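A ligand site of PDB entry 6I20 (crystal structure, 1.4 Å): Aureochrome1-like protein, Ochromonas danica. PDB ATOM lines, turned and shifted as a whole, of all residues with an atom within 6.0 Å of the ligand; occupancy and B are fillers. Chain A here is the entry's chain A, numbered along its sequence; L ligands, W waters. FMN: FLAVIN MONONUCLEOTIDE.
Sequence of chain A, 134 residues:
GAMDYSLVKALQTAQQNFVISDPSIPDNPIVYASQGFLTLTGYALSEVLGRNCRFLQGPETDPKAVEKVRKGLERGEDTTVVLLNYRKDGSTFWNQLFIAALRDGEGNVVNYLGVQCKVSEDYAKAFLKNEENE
Water W1 bridges O2P of the ligand (2.5 Å) and NE of Arg 54 (2.9 Å). Water W4 lies within hydrogen-bond range of the backbone carbonyl oxygen (O) of Asn 28, the backbone NH (N) of Cys 53, an oxygen (O2') of the ligand and the side-chain amide nitrogen (ND2) of Asn 52.
The backbone NH (N) of Arg 54 is in hydrogen-bond range of the side-chain amide oxygen (OD1) of Asn 52 (2.9 Å). The guanidinium group (NH1) of Arg 54 is in salt-bridge range of the side-chain carboxylate (OD2) of Asp 27, at 2.8 Å. ND2 of Asn 52 sits at hydrogen-bond distance from O of Asp 27 (2.9 Å). ND2 of Asn 85 lies close to O of Leu 56. O of Leu 83 lies within hydrogen-bond range of N of Asn 95, at 2.9 Å. The backbone NH (N) of Val 19 is in hydrogen-bond range of the backbone carbonyl oxygen (O) of Gly 114, 2.9 Å away. The side-chain hydroxyl (OG) of Ser 21 lies within hydrogen-bond range of the side-chain amide oxygen (OD1) of Asn 28, 2.7 Å away. The backbone NH of Ser 21 is in hydrogen-bond range of the backbone carbonyl oxygen of Tyr 112, 2.9 Å away.
Residues that only touch the ligand: Val 66 (3.4 Å), Gly 114 (3.5 Å), Asn 28 (3.5 Å), Leu 73 (3.5 Å), Leu 97 (3.6 Å), Ser 21 (3.6 Å), Leu 56 (3.6 Å), Val 19 (3.6 Å), Ile 99 (3.6 Å), Leu 83 (3.6 Å), Tyr 112 (3.7 Å), Leu 113 (3.7 Å) and Val 69 (3.9 Å). Within 4 Å of the ligand: Val 19, Ser 21, Asn 28, Asn 52, Cys 53, Arg 54, Leu 56, Gln 57, Val 66, Val 69, Arg 70, Leu 73, Leu 83, Asn 85, Asn 95, Leu 97, Ile 99, Tyr 112, Leu 113, Gly 114 and Gln 116.
O2P of the ligand lies within salt-bridge range of NH1 of Arg 70 (2.6 Å). The guanidinium group (NH2) of Arg 54 is in salt-bridge range of an oxygen (O1P) of the ligand (2.7 Å). O2' of the ligand lies within hydrogen-bond range of OD1 of Asn 52 (2.8 Å). A nitrogen (N3) of the ligand sits at hydrogen-bond distance from the side-chain amide oxygen (OD1) of Asn 85 (2.9 Å). An oxygen (O4') of the ligand sits at hydrogen-bond distance from the side-chain amide nitrogen (NE2) of Gln 57 (3.0 Å). NE2 of Gln 116 is in hydrogen-bond range of O4 of the ligand. An oxygen (O4) of the ligand sits at hydrogen-bond distance from the side-chain amide nitrogen of Asn 95 (3.1 Å). N5 of the ligand sits at hydrogen-bond distance from SG of Cys 53 (3.4 Å).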
ATOM      1  N   VAL A  19      23.591  15.510 -17.175  1.00  0.00           N
ATOM      2  CA  VAL A  19      22.844  14.760 -16.189  1.00  0.00           C
ATOM      3  C   VAL A  19      21.756  15.641 -15.606  1.00  0.00           C
ATOM      4  O   VAL A  19      21.819  16.870 -15.688  1.00  0.00           O
ATOM      5  CB  VAL A  19      23.716  14.243 -15.017  1.00  0.00           C
ATOM      6  CG1 VAL A  19      24.791  13.310 -15.537  1.00  0.00           C
ATOM      7  CG2 VAL A  19      24.312  15.355 -14.231  1.00  0.00           C
ATOM      8  N   ILE A  20      20.745  14.993 -15.043  1.00  0.00           N
ATOM      9  CA  ILE A  20      19.670  15.637 -14.291  1.00  0.00           C
ATOM     10  C   ILE A  20      19.706  15.061 -12.877  1.00  0.00           C
ATOM     11  O   ILE A  20      19.763  13.821 -12.733  1.00  0.00           O
ATOM     12  CB  ILE A  20      18.286  15.314 -14.927  1.00  0.00           C
ATOM     13  CG1 ILE A  20      18.309  15.627 -16.424  1.00  0.00           C
ATOM     14  CG2 ILE A  20      17.208  16.108 -14.209  1.00  0.00           C
ATOM     15  CD1 ILE A  20      18.609  17.073 -16.734  1.00  0.00           C
ATOM     16  N   SER A  21      19.666  15.929 -11.854  1.00  0.00           N
ATOM     17  CA  SER A  21      19.619  15.476 -10.465  1.00  0.00           C
ATOM     18  C   SER A  21      18.275  15.839  -9.848  1.00  0.00           C
ATOM     19  O   SER A  21      17.532  16.667 -10.396  1.00  0.00           O
ATOM     20  CB  SER A  21      20.735  16.090  -9.621  1.00  0.00           C
ATOM     21  OG  SER A  21      20.447  17.443  -9.273  1.00  0.00           O
ATOM     22  N   ASP A  27      20.832  13.434  -0.868  1.00  0.00           N
ATOM     23  CA  ASP A  27      22.089  13.696  -1.507  1.00  0.00           C
ATOM     24  C   ASP A  27      22.019  14.108  -2.973  1.00  0.00           C
ATOM     25  O   ASP A  27      23.014  14.044  -3.676  1.00  0.00           O
ATOM     26  CB  ASP A  27      23.071  12.512  -1.353  1.00  0.00           C
ATOM     27  CG  ASP A  27      24.524  12.968  -1.344  1.00  0.00           C
ATOM     28  OD1 ASP A  27      24.793  14.174  -1.090  1.00  0.00           O
ATOM     29  OD2 ASP A  27      25.422  12.111  -1.596  1.00  0.00           O
ATOM     30  N   ASN A  28      20.856  14.571  -3.402  1.00  0.00           N
ATOM     31  CA  ASN A  28      20.715  15.175  -4.722  1.00  0.00           C
ATOM     32  C   ASN A  28      21.331  14.346  -5.844  1.00  0.00           C
ATOM     33  O   ASN A  28      22.213  14.831  -6.612  1.00  0.00           O
ATOM     34  CB  ASN A  28      21.319  16.602  -4.705  1.00  0.00           C
ATOM     35  CG  ASN A  28      21.007  17.416  -5.933  1.00  0.00           C
ATOM     36  OD1 ASN A  28      19.991  17.212  -6.613  1.00  0.00           O
ATOM     37  ND2 ASN A  28      21.891  18.351  -6.231  1.00  0.00           N
ATOM     38  N   PHE A  37      27.536  11.701 -21.489  1.00  0.00           N
ATOM     39  CA  PHE A  37      28.112  11.705 -20.137  1.00  0.00           C
ATOM     40  C   PHE A  37      28.756  10.358 -19.824  1.00  0.00           C
ATOM     41  O   PHE A  37      29.872  10.284 -19.275  1.00  0.00           O
ATOM     42  CB  PHE A  37      27.062  12.008 -19.096  1.00  0.00           C
ATOM     43  CG  PHE A  37      27.551  11.990 -17.670  1.00  0.00           C
ATOM     44  CD1 PHE A  37      28.111  13.129 -17.105  1.00  0.00           C
ATOM     45  CD2 PHE A  37      27.412  10.857 -16.905  1.00  0.00           C
ATOM     46  CE1 PHE A  37      28.559  13.120 -15.788  1.00  0.00           C
ATOM     47  CE2 PHE A  37      27.859  10.866 -15.588  1.00  0.00           C
ATOM     48  CZ  PHE A  37      28.417  11.976 -15.030  1.00  0.00           C
ATOM     49  N   ASN A  52      25.304  10.918  -6.303  1.00  0.00           N
ATOM     50  CA  ASN A  52      25.713  12.312  -6.451  1.00  0.00           C
ATOM     51  C   ASN A  52      26.925  12.376  -7.369  1.00  0.00           C
ATOM     52  O   ASN A  52      27.854  11.554  -7.266  1.00  0.00           O
ATOM     53  CB  ASN A  52      26.052  12.904  -5.079  1.00  0.00           C
ATOM     54  CG  ASN A  52      26.363  14.367  -5.147  1.00  0.00           C
ATOM     55  OD1 ASN A  52      27.445  14.740  -5.588  1.00  0.00           O
ATOM     56  ND2 ASN A  52      25.401  15.197  -4.728  1.00  0.00           N
ATOM     57  N   CYS A  53      26.973  13.388  -8.232  1.00  0.00           N
ATOM     58  CA  CYS A  53      28.034  13.519  -9.248  1.00  0.00           C
ATOM     59  C   CYS A  53      29.482  13.800  -8.695  1.00  0.00           C
ATOM     60  O   CYS A  53      30.442  13.768  -9.463  1.00  0.00           O
ATOM     61  CB  CYS A  53      27.592  14.551 -10.318  1.00  0.00           C
ATOM     62  SG  CYS A  53      27.981  14.110 -12.008  1.00  0.00           S
ATOM     63  N   ARG A  54      29.608  13.987  -7.378  1.00  0.00           N
ATOM     64  CA  ARG A  54      30.911  14.207  -6.804  1.00  0.00           C
ATOM     65  C   ARG A  54      31.857  13.046  -7.013  1.00  0.00           C
ATOM     66  O   ARG A  54      33.053  13.180  -6.763  1.00  0.00           O
ATOM     67  CB  ARG A  54      30.828  14.550  -5.319  1.00  0.00           C
ATOM     68  CG  ARG A  54      30.562  13.376  -4.419  1.00  0.00           C
ATOM     69  CD  ARG A  54      30.646  13.751  -2.947  1.00  0.00           C
ATOM     70  NE  ARG A  54      29.582  14.628  -2.519  1.00  0.00           N
ATOM     71  CZ  ARG A  54      28.364  14.224  -2.191  1.00  0.00           C
ATOM     72  NH1 ARG A  54      28.009  12.950  -2.202  1.00  0.00           N
ATOM     73  NH2 ARG A  54      27.446  15.132  -1.848  1.00  0.00           N
ATOM     74  N   LEU A  56      33.020  12.124  -9.589  1.00  0.00           N
ATOM     75  CA  LEU A  56      33.968  12.608 -10.616  1.00  0.00           C
ATOM     76  C   LEU A  56      35.139  13.382 -10.066  1.00  0.00           C
ATOM     77  O   LEU A  56      36.083  13.674 -10.784  1.00  0.00           O
ATOM     78  CB  LEU A  56      33.234  13.427 -11.673  1.00  0.00           C
ATOM     79  CG  LEU A  56      32.213  12.691 -12.499  1.00  0.00           C
ATOM     80  CD1 LEU A  56      31.549  13.658 -13.481  1.00  0.00           C
ATOM     81  CD2 LEU A  56      32.815  11.519 -13.270  1.00  0.00           C
ATOM     82  N   GLN A  57      35.107  13.705  -8.763  1.00  0.00           N
ATOM     83  CA  GLN A  57      36.159  14.530  -8.176  1.00  0.00           C
ATOM     84  C   GLN A  57      37.239  13.674  -7.535  1.00  0.00           C
ATOM     85  O   GLN A  57      36.984  12.537  -7.151  1.00  0.00           O
ATOM     86  CB  GLN A  57      35.542  15.464  -7.153  1.00  0.00           C
ATOM     87  CG  GLN A  57      34.492  16.409  -7.757  1.00  0.00           C
ATOM     88  CD  GLN A  57      33.584  17.049  -6.742  1.00  0.00           C
ATOM     89  OE1 GLN A  57      33.834  17.007  -5.520  1.00  0.00           O
ATOM     90  NE2 GLN A  57      32.501  17.691  -7.244  1.00  0.00           N
ATOM     91  N   THR A  61      41.337  17.822  -7.856  1.00  0.00           N
ATOM     92  CA  THR A  61      40.214  18.749  -8.046  1.00  0.00           C
ATOM     93  C   THR A  61      40.312  19.879  -7.036  1.00  0.00           C
ATOM     94  O   THR A  61      40.542  19.639  -5.859  1.00  0.00           O
ATOM     95  CB  THR A  61      38.889  18.005  -7.825  1.00  0.00           C
ATOM     96  OG1 THR A  61      38.822  16.859  -8.670  1.00  0.00           O
ATOM     97  CG2 THR A  61      37.691  18.905  -8.104  1.00  0.00           C
ATOM     98  N   VAL A  66      34.641  23.380  -6.263  1.00  0.00           N
ATOM     99  CA  VAL A  66      33.500  22.655  -5.714  1.00  0.00           C
ATOM    100  C   VAL A  66      32.633  23.576  -4.837  1.00  0.00           C
ATOM    101  O   VAL A  66      31.397  23.525  -4.876  1.00  0.00           O
ATOM    102  CB  VAL A  66      34.002  21.391  -4.940  1.00  0.00           C
ATOM    103  CG1 VAL A  66      32.864  20.655  -4.263  1.00  0.00           C
ATOM    104  CG2 VAL A  66      34.726  20.480  -5.908  1.00  0.00           C
ATOM    105  N   VAL A  69      30.319  25.682  -6.946  1.00  0.00           N
ATOM    106  CA  VAL A  69      29.157  24.902  -7.326  1.00  0.00           C
ATOM    107  C   VAL A  69      28.161  24.855  -6.157  1.00  0.00           C
ATOM    108  O   VAL A  69      26.945  25.060  -6.313  1.00  0.00           O
ATOM    109  CB  VAL A  69      29.528  23.502  -7.812  1.00  0.00           C
ATOM    110  CG1 VAL A  69      28.284  22.665  -7.969  1.00  0.00           C
ATOM    111  CG2 VAL A  69      30.353  23.546  -9.096  1.00  0.00           C
ATOM    112  N   ARG A  70      28.686  24.532  -4.972  1.00  0.00           N
ATOM    113  CA  ARG A  70      27.845  24.418  -3.803  1.00  0.00           C
ATOM    114  C   ARG A  70      27.059  25.681  -3.550  1.00  0.00           C
ATOM    115  O   ARG A  70      25.865  25.620  -3.261  1.00  0.00           O
ATOM    116  CB  ARG A  70      28.756  24.077  -2.614  1.00  0.00           C
ATOM    117  CG  ARG A  70      28.081  23.665  -1.325  1.00  0.00           C
ATOM    118  CD  ARG A  70      29.165  23.357  -0.291  1.00  0.00           C
ATOM    119  NE  ARG A  70      29.879  22.108  -0.604  1.00  0.00           N
ATOM    120  CZ  ARG A  70      31.201  21.904  -0.782  1.00  0.00           C
ATOM    121  NH1 ARG A  70      31.622  20.668  -1.059  1.00  0.00           N
ATOM    122  NH2 ARG A  70      32.114  22.874  -0.696  1.00  0.00           N
ATOM    123  N   LEU A  73      24.159  26.293  -5.959  1.00  0.00           N
ATOM    124  CA  LEU A  73      23.042  25.466  -5.544  1.00  0.00           C
ATOM    125  C   LEU A  73      22.316  26.041  -4.308  1.00  0.00           C
ATOM    126  O   LEU A  73      21.071  26.012  -4.284  1.00  0.00           O
ATOM    127  CB  LEU A  73      23.518  24.029  -5.289  1.00  0.00           C
ATOM    128  CG  LEU A  73      23.981  23.237  -6.503  1.00  0.00           C
ATOM    129  CD1 LEU A  73      24.665  21.915  -6.110  1.00  0.00           C
ATOM    130  CD2 LEU A  73      22.870  22.913  -7.458  1.00  0.00           C
ATOM    131  N   GLU A  74      23.043  26.522  -3.307  1.00  0.00           N
ATOM    132  CA  GLU A  74      22.454  27.070  -2.087  1.00  0.00           C
ATOM    133  C   GLU A  74      21.721  28.412  -2.340  1.00  0.00           C
ATOM    134  O   GLU A  74      20.696  28.694  -1.701  1.00  0.00           O
ATOM    135  CB  GLU A  74      23.514  27.188  -0.958  1.00  0.00           C
ATOM    136  CG  GLU A  74      23.718  25.849  -0.199  1.00  0.00           C
ATOM    137  CD  GLU A  74      25.116  25.549   0.348  1.00  0.00           C
ATOM    138  OE1 GLU A  74      25.935  26.484   0.542  1.00  0.00           O
ATOM    139  OE2 GLU A  74      25.407  24.344   0.624  1.00  0.00           O
ATOM    140  N   LEU A  83      36.734  22.642 -13.677  1.00  0.00           N
ATOM    141  CA  LEU A  83      37.405  21.854 -12.630  1.00  0.00           C
ATOM    142  C   LEU A  83      37.885  20.547 -13.189  1.00  0.00           C
ATOM    143  O   LEU A  83      37.401  20.032 -14.185  1.00  0.00           O
ATOM    144  CB  LEU A  83      36.516  21.685 -11.407  1.00  0.00           C
ATOM    145  CG  LEU A  83      35.467  20.575 -11.401  1.00  0.00           C
ATOM    146  CD1 LEU A  83      34.749  20.536 -10.048  1.00  0.00           C
ATOM    147  CD2 LEU A  83      34.425  20.706 -12.498  1.00  0.00           C
ATOM    148  N   LEU A  84      38.881  19.969 -12.478  1.00  0.00           N
ATOM    149  CA  LEU A  84      39.442  18.695 -12.877  1.00  0.00           C
ATOM    150  C   LEU A  84      38.561  17.552 -12.410  1.00  0.00           C
ATOM    151  O   LEU A  84      38.170  17.514 -11.239  1.00  0.00           O
ATOM    152  CB  LEU A  84      40.845  18.562 -12.300  1.00  0.00           C
ATOM    153  CG  LEU A  84      41.678  17.442 -12.925  1.00  0.00           C
ATOM    154  CD1 LEU A  84      42.155  17.820 -14.323  1.00  0.00           C
ATOM    155  CD2 LEU A  84      42.870  17.088 -12.027  1.00  0.00           C
ATOM    156  N   ASN A  85      38.237  16.652 -13.323  1.00  0.00           N
ATOM    157  CA  ASN A  85      37.434  15.485 -13.001  1.00  0.00           C
ATOM    158  C   ASN A  85      38.201  14.228 -13.460  1.00  0.00           C
ATOM    159  O   ASN A  85      39.183  14.279 -14.177  1.00  0.00           O
ATOM    160  CB  ASN A  85      36.065  15.533 -13.690  1.00  0.00           C
ATOM    161  CG  ASN A  85      35.008  16.334 -12.978  1.00  0.00           C
ATOM    162  OD1 ASN A  85      33.877  16.395 -13.528  1.00  0.00           O
ATOM    163  ND2 ASN A  85      35.232  16.857 -11.775  1.00  0.00           N
ATOM    164  N   ASN A  95      36.799  19.853 -16.997  1.00  0.00           N
ATOM    165  CA  ASN A  95      35.364  19.890 -17.244  1.00  0.00           C
ATOM    166  C   ASN A  95      34.907  21.339 -17.059  1.00  0.00           C
ATOM    167  O   ASN A  95      34.971  21.876 -15.962  1.00  0.00           O
ATOM    168  CB  ASN A  95      34.685  18.970 -16.220  1.00  0.00           C
ATOM    169  CG  ASN A  95      33.184  18.887 -16.315  1.00  0.00           C
ATOM    170  OD1 ASN A  95      32.554  19.544 -17.155  1.00  0.00           O
ATOM    171  ND2 ASN A  95      32.579  18.047 -15.478  1.00  0.00           N
ATOM    172  N   LEU A  97      31.778  22.974 -16.520  1.00  0.00           N
ATOM    173  CA  LEU A  97      30.544  22.464 -15.989  1.00  0.00           C
ATOM    174  C   LEU A  97      29.551  23.606 -15.810  1.00  0.00           C
ATOM    175  O   LEU A  97      29.852  24.586 -15.195  1.00  0.00           O
ATOM    176  CB  LEU A  97      30.826  21.839 -14.612  1.00  0.00           C
ATOM    177  CG  LEU A  97      29.647  21.372 -13.816  1.00  0.00           C
ATOM    178  CD1 LEU A  97      28.848  20.267 -14.498  1.00  0.00           C
ATOM    179  CD2 LEU A  97      30.114  20.885 -12.437  1.00  0.00           C
ATOM    180  N   PHE A  98      28.357  23.409 -16.372  1.00  0.00           N
ATOM    181  CA  PHE A  98      27.229  24.352 -16.215  1.00  0.00           C
ATOM    182  C   PHE A  98      26.154  23.672 -15.394  1.00  0.00           C
ATOM    183  O   PHE A  98      25.750  22.546 -15.732  1.00  0.00           O
ATOM    184  CB  PHE A  98      26.649  24.614 -17.622  1.00  0.00           C
ATOM    185  CG  PHE A  98      25.298  25.303 -17.634  1.00  0.00           C
ATOM    186  CD1 PHE A  98      25.119  26.517 -17.012  1.00  0.00           C
ATOM    187  CD2 PHE A  98      24.231  24.726 -18.284  1.00  0.00           C
ATOM    188  CE1 PHE A  98      23.875  27.154 -17.068  1.00  0.00           C
ATOM    189  CE2 PHE A  98      23.008  25.370 -18.346  1.00  0.00           C
ATOM    190  CZ  PHE A  98      22.826  26.555 -17.717  1.00  0.00           C
ATOM    191  N   ILE A  99      25.673  24.353 -14.351  1.00  0.00           N
ATOM    192  CA  ILE A  99      24.571  23.803 -13.551  1.00  0.00           C
ATOM    193  C   ILE A  99      23.486  24.842 -13.455  1.00  0.00           C
ATOM    194  O   ILE A  99      23.745  26.029 -13.223  1.00  0.00           O
ATOM    195  CB  ILE A  99      25.029  23.309 -12.144  1.00  0.00           C
ATOM    196  CG1 ILE A  99      26.142  22.272 -12.295  1.00  0.00           C
ATOM    197  CG2 ILE A  99      23.875  22.699 -11.361  1.00  0.00           C
ATOM    198  CD1 ILE A  99      26.833  21.924 -10.975  1.00  0.00           C
ATOM    199  N   TYR A 112      17.885  19.714 -11.089  1.00  0.00           N
ATOM    200  CA  TYR A 112      19.008  20.460 -11.625  1.00  0.00           C
ATOM    201  C   TYR A 112      19.540  19.794 -12.877  1.00  0.00           C
ATOM    202  O   TYR A 112      19.539  18.562 -12.984  1.00  0.00           O
ATOM    203  CB  TYR A 112      20.162  20.549 -10.613  1.00  0.00           C
ATOM    204  CG  TYR A 112      19.804  21.369  -9.407  1.00  0.00           C
ATOM    205  CD1 TYR A 112      19.849  22.748  -9.446  1.00  0.00           C
ATOM    206  CD2 TYR A 112      19.479  20.780  -8.202  1.00  0.00           C
ATOM    207  CE1 TYR A 112      19.504  23.511  -8.347  1.00  0.00           C
ATOM    208  CE2 TYR A 112      19.146  21.544  -7.095  1.00  0.00           C
ATOM    209  CZ  TYR A 112      19.136  22.897  -7.165  1.00  0.00           C
ATOM    210  OH  TYR A 112      18.786  23.649  -6.044  1.00  0.00           O
ATOM    211  N   LEU A 113      19.969  20.636 -13.821  1.00  0.00           N
ATOM    212  CA  LEU A 113      20.617  20.208 -15.024  1.00  0.00           C
ATOM    213  C   LEU A 113      22.097  20.491 -14.887  1.00  0.00           C
ATOM    214  O   LEU A 113      22.471  21.586 -14.473  1.00  0.00           O
ATOM    215  CB  LEU A 113      20.072  21.037 -16.207  1.00  0.00           C
ATOM    216  CG  LEU A 113      20.768  20.878 -17.547  1.00  0.00           C
ATOM    217  CD1 LEU A 113      20.601  19.466 -18.060  1.00  0.00           C
ATOM    218  CD2 LEU A 113      20.216  21.898 -18.538  1.00  0.00           C
ATOM    219  N   GLY A 114      22.934  19.527 -15.270  1.00  0.00           N
ATOM    220  CA  GLY A 114      24.365  19.756 -15.341  1.00  0.00           C
ATOM    221  C   GLY A 114      24.872  19.338 -16.693  1.00  0.00           C
ATOM    222  O   GLY A 114      24.566  18.241 -17.160  1.00  0.00           O
ATOM    223  N   VAL A 115      25.576  20.235 -17.361  1.00  0.00           N
ATOM    224  CA  VAL A 115      26.113  19.986 -18.696  1.00  0.00           C
ATOM    225  C   VAL A 115      27.629  20.052 -18.636  1.00  0.00           C
ATOM    226  O   VAL A 115      28.186  21.058 -18.186  1.00  0.00           O
ATOM    227  CB  VAL A 115      25.573  21.024 -19.721  1.00  0.00           C
ATOM    228  CG1 VAL A 115      26.187  20.779 -21.109  1.00  0.00           C
ATOM    229  CG2 VAL A 115      24.032  21.020 -19.746  1.00  0.00           C
ATOM    230  N   GLN A 116      28.295  18.986 -19.085  1.00  0.00           N
ATOM    231  CA  GLN A 116      29.738  18.869 -18.988  1.00  0.00           C
ATOM    232  C   GLN A 116      30.363  19.058 -20.365  1.00  0.00           C
ATOM    233  O   GLN A 116      29.936  18.454 -21.338  1.00  0.00           O
ATOM    234  CB  GLN A 116      30.144  17.484 -18.460  1.00  0.00           C
ATOM    235  CG  GLN A 116      29.637  17.208 -17.063  1.00  0.00           C
ATOM    236  CD  GLN A 116      28.212  16.724 -16.930  1.00  0.00           C
ATOM    237  OE1 GLN A 116      27.548  16.338 -17.906  1.00  0.00           O
ATOM    238  NE2 GLN A 116      27.709  16.692 -15.651  1.00  0.00           N
HETATM  239  N1  FMN L   1      30.604  17.879  -9.947  1.00  0.00           N
HETATM  240  C2  FMN L   1      31.633  17.522 -10.742  1.00  0.00           C
HETATM  241  O2  FMN L   1      32.786  17.486 -10.254  1.00  0.00           O
HETATM  242  N3  FMN L   1      31.466  17.176 -12.047  1.00  0.00           N
HETATM  243  C4  FMN L   1      30.246  17.192 -12.651  1.00  0.00           C
HETATM  244  O4  FMN L   1      30.144  16.936 -13.883  1.00  0.00           O
HETATM  245  C4A FMN L   1      29.120  17.526 -11.847  1.00  0.00           C
HETATM  246  N5  FMN L   1      27.864  17.534 -12.382  1.00  0.00           N
HETATM  247  C5A FMN L   1      26.840  17.949 -11.587  1.00  0.00           C
HETATM  248  C6  FMN L   1      25.537  18.000 -12.117  1.00  0.00           C
HETATM  249  C7  FMN L   1      24.476  18.401 -11.366  1.00  0.00           C
HETATM  250  C7M FMN L   1      23.056  18.475 -11.979  1.00  0.00           C
HETATM  251  C8  FMN L   1      24.658  18.788  -9.995  1.00  0.00           C
HETATM  252  C8M FMN L   1      23.503  19.254  -9.170  1.00  0.00           C
HETATM  253  C9  FMN L   1      25.923  18.752  -9.460  1.00  0.00           C
HETATM  254  C9A FMN L   1      27.021  18.370 -10.216  1.00  0.00           C
HETATM  255  N10 FMN L   1      28.312  18.266  -9.638  1.00  0.00           N
HETATM  256  C10 FMN L   1      29.358  17.922 -10.460  1.00  0.00           C
HETATM  257  C1' FMN L   1      28.592  18.757  -8.297  1.00  0.00           C
HETATM  258  C2' FMN L   1      28.438  17.732  -7.164  1.00  0.00           C
HETATM  259  O2' FMN L   1      27.343  16.863  -7.484  1.00  0.00           O
HETATM  260  C3' FMN L   1      28.134  18.463  -5.865  1.00  0.00           C
HETATM  261  O3' FMN L   1      26.987  19.319  -5.986  1.00  0.00           O
HETATM  262  C4' FMN L   1      29.282  19.281  -5.308  1.00  0.00           C
HETATM  263  O4' FMN L   1      30.434  18.420  -5.223  1.00  0.00           O
HETATM  264  C5' FMN L   1      28.950  19.796  -3.870  1.00  0.00           C
HETATM  265  O5' FMN L   1      28.217  18.770  -3.119  1.00  0.00           O
HETATM  266  P   FMN L   1      28.323  18.834  -1.513  1.00  0.00           P
HETATM  267  O1P FMN L   1      27.577  17.663  -1.004  1.00  0.00           O
HETATM  268  O2P FMN L   1      29.767  18.797  -1.189  1.00  0.00           O
HETATM  269  O3P FMN L   1      27.688  20.174  -1.161  1.00  0.00           O
HETATM  270  O   HOH W   1      30.795  17.275  -2.855  1.00  0.00           O
HETATM  271  O   HOH W   2      25.614  20.874  -2.666  1.00  0.00           O
HETATM  272  O   HOH W   3      26.072  17.514   1.407  1.00  0.00           O
HETATM  273  O   HOH W   4      24.651  15.289  -8.091  1.00  0.00           O
